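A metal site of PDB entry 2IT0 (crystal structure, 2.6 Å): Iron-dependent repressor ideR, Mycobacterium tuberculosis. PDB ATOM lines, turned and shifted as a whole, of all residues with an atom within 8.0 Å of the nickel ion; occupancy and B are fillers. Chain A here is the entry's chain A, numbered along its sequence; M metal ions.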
ATOM      1  N   GLU A   3      30.887  -4.241  -2.382  1.00  0.00           N
ATOM      2  CA  GLU A   3      30.184  -3.232  -1.526  1.00  0.00           C
ATOM      3  C   GLU A   3      28.744  -3.650  -1.190  1.00  0.00           C
ATOM      4  O   GLU A   3      28.331  -3.640  -0.023  1.00  0.00           O
ATOM      5  CB  GLU A   3      30.145  -1.881  -2.219  1.00  0.00           C
ATOM      6  CG  GLU A   3      29.365  -0.848  -1.437  1.00  0.00           C
ATOM      7  CD  GLU A   3      30.263  -0.038  -0.536  1.00  0.00           C
ATOM      8  OE1 GLU A   3      30.199  -0.243   0.705  1.00  0.00           O
ATOM      9  OE2 GLU A   3      31.039   0.796  -1.073  1.00  0.00           O
ATOM     10  N   LEU A   4      27.981  -3.972  -2.226  1.00  0.00           N
ATOM     11  CA  LEU A   4      26.628  -4.473  -2.069  1.00  0.00           C
ATOM     12  C   LEU A   4      26.665  -5.985  -1.981  1.00  0.00           C
ATOM     13  O   LEU A   4      25.650  -6.632  -1.748  1.00  0.00           O
ATOM     14  CB  LEU A   4      25.782  -4.062  -3.266  1.00  0.00           C
ATOM     15  CG  LEU A   4      25.481  -2.582  -3.447  1.00  0.00           C
ATOM     16  CD1 LEU A   4      24.884  -2.368  -4.819  1.00  0.00           C
ATOM     17  CD2 LEU A   4      24.533  -2.082  -2.352  1.00  0.00           C
ATOM     18  N   VAL A   5      27.864  -6.532  -2.165  1.00  0.00           N
ATOM     19  CA  VAL A   5      28.108  -7.978  -2.179  1.00  0.00           C
ATOM     20  C   VAL A   5      27.545  -8.625  -3.456  1.00  0.00           C
ATOM     21  O   VAL A   5      28.256  -9.338  -4.127  1.00  0.00           O
ATOM     22  CB  VAL A   5      27.637  -8.714  -0.880  1.00  0.00           C
ATOM     23  CG1 VAL A   5      28.072 -10.162  -0.910  1.00  0.00           C
ATOM     24  CG2 VAL A   5      28.186  -8.014   0.353  1.00  0.00           C
ATOM     25  N   ASP A   6      26.288  -8.360  -3.773  1.00  0.00           N
ATOM     26  CA  ASP A   6      25.707  -8.776  -5.057  1.00  0.00           C
ATOM     27  C   ASP A   6      24.716  -7.709  -5.509  1.00  0.00           C
ATOM     28  O   ASP A   6      23.664  -7.543  -4.906  1.00  0.00           O
ATOM     29  CB  ASP A   6      25.010 -10.136  -4.931  1.00  0.00           C
ATOM     30  CG  ASP A   6      24.487 -10.665  -6.277  1.00  0.00           C
ATOM     31  OD1 ASP A   6      23.887 -11.748  -6.301  1.00  0.00           O
ATOM     32  OD2 ASP A   6      24.671 -10.001  -7.313  1.00  0.00           O
ATOM     33  N   THR A   7      25.075  -6.976  -6.573  1.00  0.00           N
ATOM     34  CA  THR A   7      24.265  -5.851  -7.040  1.00  0.00           C
ATOM     35  C   THR A   7      22.834  -6.275  -7.357  1.00  0.00           C
ATOM     36  O   THR A   7      21.875  -5.774  -6.769  1.00  0.00           O
ATOM     37  CB  THR A   7      24.875  -5.145  -8.283  1.00  0.00           C
ATOM     38  OG1 THR A   7      26.154  -4.605  -7.966  1.00  0.00           O
ATOM     39  CG2 THR A   7      23.986  -4.015  -8.718  1.00  0.00           C
ATOM     40  N   GLU A   9      20.869  -8.827  -6.689  1.00  0.00           N
ATOM     41  CA  GLU A   9      20.028  -9.172  -5.543  1.00  0.00           C
ATOM     42  C   GLU A   9      19.639  -7.969  -4.708  1.00  0.00           C
ATOM     43  O   GLU A   9      18.545  -7.923  -4.135  1.00  0.00           O
ATOM     44  CB  GLU A   9      20.703 -10.226  -4.657  1.00  0.00           C
ATOM     45  CG  GLU A   9      20.640 -11.602  -5.277  1.00  0.00           C
ATOM     46  CD  GLU A   9      21.407 -12.626  -4.479  1.00  0.00           C
ATOM     47  OE1 GLU A   9      21.981 -12.261  -3.433  1.00  0.00           O
ATOM     48  OE2 GLU A   9      21.441 -13.803  -4.918  1.00  0.00           O
ATOM     49  N   MET A  10      20.505  -6.970  -4.644  1.00  0.00           N
ATOM     50  CA  MET A  10      20.161  -5.814  -3.838  1.00  0.00           C
ATOM     51  C   MET A  10      19.086  -5.011  -4.527  1.00  0.00           C
ATOM     52  O   MET A  10      18.122  -4.563  -3.902  1.00  0.00           O
ATOM     53  CB  MET A  10      21.404  -4.997  -3.487  1.00  0.00           C
ATOM     54  CG  MET A  10      22.171  -5.590  -2.309  1.00  0.00           C
ATOM     55  SD  MET A  10      21.215  -5.499  -0.765  1.00  0.00           S
ATOM     56  CE  MET A  10      21.635  -3.854  -0.218  1.00  0.00           C
ATOM     57  N   TYR A  11      19.225  -4.867  -5.840  1.00  0.00           N
ATOM     58  CA  TYR A  11      18.174  -4.245  -6.635  1.00  0.00           C
ATOM     59  C   TYR A  11      16.842  -4.951  -6.423  1.00  0.00           C
ATOM     60  O   TYR A  11      15.874  -4.327  -5.991  1.00  0.00           O
ATOM     61  CB  TYR A  11      18.561  -4.242  -8.096  1.00  0.00           C
ATOM     62  CG  TYR A  11      19.450  -3.087  -8.466  1.00  0.00           C
ATOM     63  CD1 TYR A  11      20.531  -2.734  -7.662  1.00  0.00           C
ATOM     64  CD2 TYR A  11      19.213  -2.338  -9.609  1.00  0.00           C
ATOM     65  CE1 TYR A  11      21.350  -1.685  -7.995  1.00  0.00           C
ATOM     66  CE2 TYR A  11      20.026  -1.277  -9.954  1.00  0.00           C
ATOM     67  CZ  TYR A  11      21.094  -0.946  -9.147  1.00  0.00           C
ATOM     68  OH  TYR A  11      21.909   0.103  -9.471  1.00  0.00           O
ATOM     69  N   ARG A  13      15.817  -6.942  -4.140  1.00  0.00           N
ATOM     70  CA  ARG A  13      15.335  -6.831  -2.762  1.00  0.00           C
ATOM     71  C   ARG A  13      14.828  -5.423  -2.515  1.00  0.00           C
ATOM     72  O   ARG A  13      13.828  -5.233  -1.833  1.00  0.00           O
ATOM     73  CB  ARG A  13      16.442  -7.207  -1.767  1.00  0.00           C
ATOM     74  CG  ARG A  13      15.950  -7.797  -0.419  1.00  0.00           C
ATOM     75  CD  ARG A  13      15.956  -6.775   0.711  1.00  0.00           C
ATOM     76  NE  ARG A  13      17.312  -6.496   1.178  1.00  0.00           N
ATOM     77  CZ  ARG A  13      17.718  -5.315   1.630  1.00  0.00           C
ATOM     78  NH1 ARG A  13      16.879  -4.294   1.687  1.00  0.00           N
ATOM     79  NH2 ARG A  13      18.984  -5.144   2.027  1.00  0.00           N
ATOM     80  N   THR A  14      15.500  -4.419  -3.090  1.00  0.00           N
ATOM     81  CA  THR A  14      15.094  -3.049  -2.825  1.00  0.00           C
ATOM     82  C   THR A  14      13.726  -2.774  -3.440  1.00  0.00           C
ATOM     83  O   THR A  14      12.879  -2.120  -2.833  1.00  0.00           O
ATOM     84  CB  THR A  14      16.124  -2.009  -3.320  1.00  0.00           C
ATOM     85  OG1 THR A  14      17.303  -2.105  -2.518  1.00  0.00           O
ATOM     86  CG2 THR A  14      15.566  -0.594  -3.182  1.00  0.00           C
ATOM     87  N   LEU A  34      20.484   3.070  -2.234  1.00  0.00           N
ATOM     88  CA  LEU A  34      21.728   2.341  -2.372  1.00  0.00           C
ATOM     89  C   LEU A  34      22.870   3.313  -2.596  1.00  0.00           C
ATOM     90  O   LEU A  34      24.017   2.908  -2.809  1.00  0.00           O
ATOM     91  CB  LEU A  34      21.621   1.338  -3.520  1.00  0.00           C
ATOM     92  CG  LEU A  34      20.519   0.297  -3.286  1.00  0.00           C
ATOM     93  CD1 LEU A  34      20.501  -0.747  -4.389  1.00  0.00           C
ATOM     94  CD2 LEU A  34      20.676  -0.354  -1.905  1.00  0.00           C
ATOM     95  N   VAL A  75      15.701 -13.708  -1.275  1.00  0.00           N
ATOM     96  CA  VAL A  75      16.717 -12.862  -0.648  1.00  0.00           C
ATOM     97  C   VAL A  75      16.159 -12.203   0.630  1.00  0.00           C
ATOM     98  O   VAL A  75      16.780 -12.230   1.692  1.00  0.00           O
ATOM     99  CB  VAL A  75      17.251 -11.798  -1.637  1.00  0.00           C
ATOM    100  CG1 VAL A  75      18.181 -10.830  -0.936  1.00  0.00           C
ATOM    101  CG2 VAL A  75      17.968 -12.450  -2.802  1.00  0.00           C
ATOM    102  N   HIS A  79      17.339 -12.466   4.421  1.00  0.00           N
ATOM    103  CA  HIS A  79      17.629 -11.241   5.145  1.00  0.00           C
ATOM    104  C   HIS A  79      17.045 -11.327   6.558  1.00  0.00           C
ATOM    105  O   HIS A  79      17.756 -11.195   7.564  1.00  0.00           O
ATOM    106  CB  HIS A  79      17.067 -10.032   4.377  1.00  0.00           C
ATOM    107  CG  HIS A  79      17.235  -8.719   5.080  1.00  0.00           C
ATOM    108  ND1 HIS A  79      18.448  -8.073   5.171  1.00  0.00           N
ATOM    109  CD2 HIS A  79      16.340  -7.929   5.723  1.00  0.00           C
ATOM    110  CE1 HIS A  79      18.294  -6.938   5.838  1.00  0.00           C
ATOM    111  NE2 HIS A  79      17.023  -6.830   6.189  1.00  0.00           N
ATOM    112  N   HIS A  98      20.283  -5.039  10.897  1.00  0.00           N
ATOM    113  CA  HIS A  98      19.900  -4.937   9.508  1.00  0.00           C
ATOM    114  C   HIS A  98      21.138  -4.872   8.625  1.00  0.00           C
ATOM    115  O   HIS A  98      21.271  -5.643   7.679  1.00  0.00           O
ATOM    116  CB  HIS A  98      19.001  -3.724   9.273  1.00  0.00           C
ATOM    117  CG  HIS A  98      18.773  -3.441   7.826  1.00  0.00           C
ATOM    118  ND1 HIS A  98      17.916  -4.190   7.058  1.00  0.00           N
ATOM    119  CD2 HIS A  98      19.345  -2.531   7.002  1.00  0.00           C
ATOM    120  CE1 HIS A  98      17.939  -3.735   5.812  1.00  0.00           C
ATOM    121  NE2 HIS A  98      18.802  -2.727   5.756  1.00  0.00           N
ATOM    122  N   ALA A  99      22.042  -3.943   8.929  1.00  0.00           N
ATOM    123  CA  ALA A  99      23.296  -3.828   8.189  1.00  0.00           C
ATOM    124  C   ALA A  99      23.968  -5.179   8.040  1.00  0.00           C
ATOM    125  O   ALA A  99      24.314  -5.567   6.927  1.00  0.00           O
ATOM    126  CB  ALA A  99      24.236  -2.846   8.840  1.00  0.00           C
ATOM    127  N   GLU A 100      24.148  -5.896   9.140  1.00  0.00           N
ATOM    128  CA  GLU A 100      24.807  -7.191   9.045  1.00  0.00           C
ATOM    129  C   GLU A 100      24.019  -8.105   8.115  1.00  0.00           C
ATOM    130  O   GLU A 100      24.581  -8.766   7.233  1.00  0.00           O
ATOM    131  CB  GLU A 100      24.978  -7.841  10.421  1.00  0.00           C
ATOM    132  CG  GLU A 100      25.887  -9.075  10.429  1.00  0.00           C
ATOM    133  CD  GLU A 100      27.356  -8.740  10.632  1.00  0.00           C
ATOM    134  OE1 GLU A 100      27.646  -7.899  11.505  1.00  0.00           O
ATOM    135  OE2 GLU A 100      28.214  -9.337   9.949  1.00  0.00           O
ATOM    136  N   ALA A 101      22.695  -8.146   8.308  1.00  0.00           N
ATOM    137  CA  ALA A 101      21.839  -8.991   7.487  1.00  0.00           C
ATOM    138  C   ALA A 101      21.910  -8.615   6.003  1.00  0.00           C
ATOM    139  O   ALA A 101      21.922  -9.497   5.136  1.00  0.00           O
ATOM    140  CB  ALA A 101      20.405  -8.951   7.990  1.00  0.00           C
ATOM    141  N   CYS A 102      21.997  -7.324   5.729  1.00  0.00           N
ATOM    142  CA  CYS A 102      22.124  -6.826   4.368  1.00  0.00           C
ATOM    143  C   CYS A 102      23.272  -7.488   3.616  1.00  0.00           C
ATOM    144  O   CYS A 102      23.272  -7.576   2.373  1.00  0.00           O
ATOM    145  CB  CYS A 102      22.320  -5.304   4.371  1.00  0.00           C
ATOM    146  SG  CYS A 102      22.290  -4.580   2.768  1.00  0.00           S
ATOM    147  N   ARG A 103      24.266  -7.957   4.368  1.00  0.00           N
ATOM    148  CA  ARG A 103      25.379  -8.696   3.802  1.00  0.00           C
ATOM    149  C   ARG A 103      25.149 -10.204   3.851  1.00  0.00           C
ATOM    150  O   ARG A 103      25.527 -10.917   2.917  1.00  0.00           O
ATOM    151  CB  ARG A 103      26.694  -8.326   4.490  1.00  0.00           C
ATOM    152  CG  ARG A 103      27.115  -6.870   4.298  1.00  0.00           C
ATOM    153  CD  ARG A 103      28.562  -6.631   4.680  1.00  0.00           C
ATOM    154  NE  ARG A 103      28.874  -7.172   6.007  1.00  0.00           N
ATOM    155  CZ  ARG A 103      28.662  -6.510   7.138  1.00  0.00           C
ATOM    156  NH1 ARG A 103      28.978  -7.077   8.300  1.00  0.00           N
ATOM    157  NH2 ARG A 103      28.138  -5.301   7.119  1.00  0.00           N
ATOM    158  N   TRP A 104      24.543 -10.685   4.932  1.00  0.00           N
ATOM    159  CA  TRP A 104      24.286 -12.133   5.096  1.00  0.00           C
ATOM    160  C   TRP A 104      23.289 -12.665   4.070  1.00  0.00           C
ATOM    161  O   TRP A 104      23.462 -13.758   3.514  1.00  0.00           O
ATOM    162  CB  TRP A 104      23.847 -12.457   6.526  1.00  0.00           C
ATOM    163  CG  TRP A 104      24.966 -12.350   7.519  1.00  0.00           C
ATOM    164  CD1 TRP A 104      26.014 -11.486   7.463  1.00  0.00           C
ATOM    165  CD2 TRP A 104      25.149 -13.143   8.689  1.00  0.00           C
ATOM    166  NE1 TRP A 104      26.849 -11.687   8.533  1.00  0.00           N
ATOM    167  CE2 TRP A 104      26.341 -12.692   9.310  1.00  0.00           C
ATOM    168  CE3 TRP A 104      24.421 -14.172   9.293  1.00  0.00           C
ATOM    169  CZ2 TRP A 104      26.824 -13.235  10.491  1.00  0.00           C
ATOM    170  CZ3 TRP A 104      24.904 -14.725  10.473  1.00  0.00           C
ATOM    171  CH2 TRP A 104      26.102 -14.250  11.055  1.00  0.00           C
ATOM    172  N   GLU A 105      22.252 -11.875   3.801  1.00  0.00           N
ATOM    173  CA  GLU A 105      21.245 -12.218   2.800  1.00  0.00           C
ATOM    174  C   GLU A 105      21.828 -12.743   1.491  1.00  0.00           C
ATOM    175  O   GLU A 105      21.146 -13.405   0.719  1.00  0.00           O
ATOM    176  CB  GLU A 105      20.356 -11.009   2.492  1.00  0.00           C
ATOM    177  CG  GLU A 105      21.096  -9.811   1.910  1.00  0.00           C
ATOM    178  CD  GLU A 105      20.221  -8.576   1.797  1.00  0.00           C
ATOM    179  OE1 GLU A 105      18.980  -8.712   1.951  1.00  0.00           O
ATOM    180  OE2 GLU A 105      20.783  -7.473   1.556  1.00  0.00           O
ATOM    181  N   HIS A 106      23.102 -12.457   1.235  1.00  0.00           N
ATOM    182  CA  HIS A 106      23.648 -12.751  -0.089  1.00  0.00           C
ATOM    183  C   HIS A 106      24.465 -14.030  -0.070  1.00  0.00           C
ATOM    184  O   HIS A 106      24.891 -14.521  -1.115  1.00  0.00           O
ATOM    185  CB  HIS A 106      24.439 -11.544  -0.637  1.00  0.00           C
ATOM    186  CG  HIS A 106      23.679 -10.249  -0.586  1.00  0.00           C
ATOM    187  ND1 HIS A 106      22.539 -10.026  -1.326  1.00  0.00           N
ATOM    188  CD2 HIS A 106      23.899  -9.115   0.122  1.00  0.00           C
ATOM    189  CE1 HIS A 106      22.076  -8.809  -1.057  1.00  0.00           C
ATOM    190  NE2 HIS A 106      22.888  -8.241  -0.183  1.00  0.00           N
HETATM  191 NI    NI M   1      22.399  -6.612   0.912  1.00  0.00          NI
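The nickel ion is bound by the side-chain carboxylate (OE2) of Glu 105, 1.9 Å away.
The backbone carbonyl oxygen (O) of Cys 102 binds the nickel ion (2.0 Å).
The nickel ion is bound by a ring nitrogen (NE2) of His 106 (2.0 Å).
The nickel ion is bound by SD of Met 10, at 2.3 Å.
The nickel ion is bound by SG of Cys 102.
The nickel ion has five donor atoms within binding distance.
Residues that only touch the nickel ion: Arg 13 (3.9 Å).
Five residues have an atom within 4 Å of the nickel ion: Met 10, Arg 13, Cys 102, Glu 105 and His 106.
The nearest printed residue that does not touch the nickel ion is Arg 103 (4.2 Å).
The side-chain carboxylate (OE1) of Glu 105 is in salt-bridge range of the guanidinium group (NE) of Arg 13 (2.9 Å).
OE1 of Glu 105 lies within hydrogen-bond range of ND1 of His 79.
The side-chain sulfur (SG) of Cys 102 sits close to the guanidinium group (NH2) of Arg 13 (3.4 Å).
A ring nitrogen (ND1) of His 106 sits at hydrogen-bond distance from the side-chain carboxylate (OE1) of Glu 9, 3.1 Å away.
The side-chain sulfur of Met 10 lies close to the guanidinium group of Arg 13, at 3.6 Å.
O of Met 10 is in hydrogen-bond range of OG1 of Thr 14 (2.9 Å).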
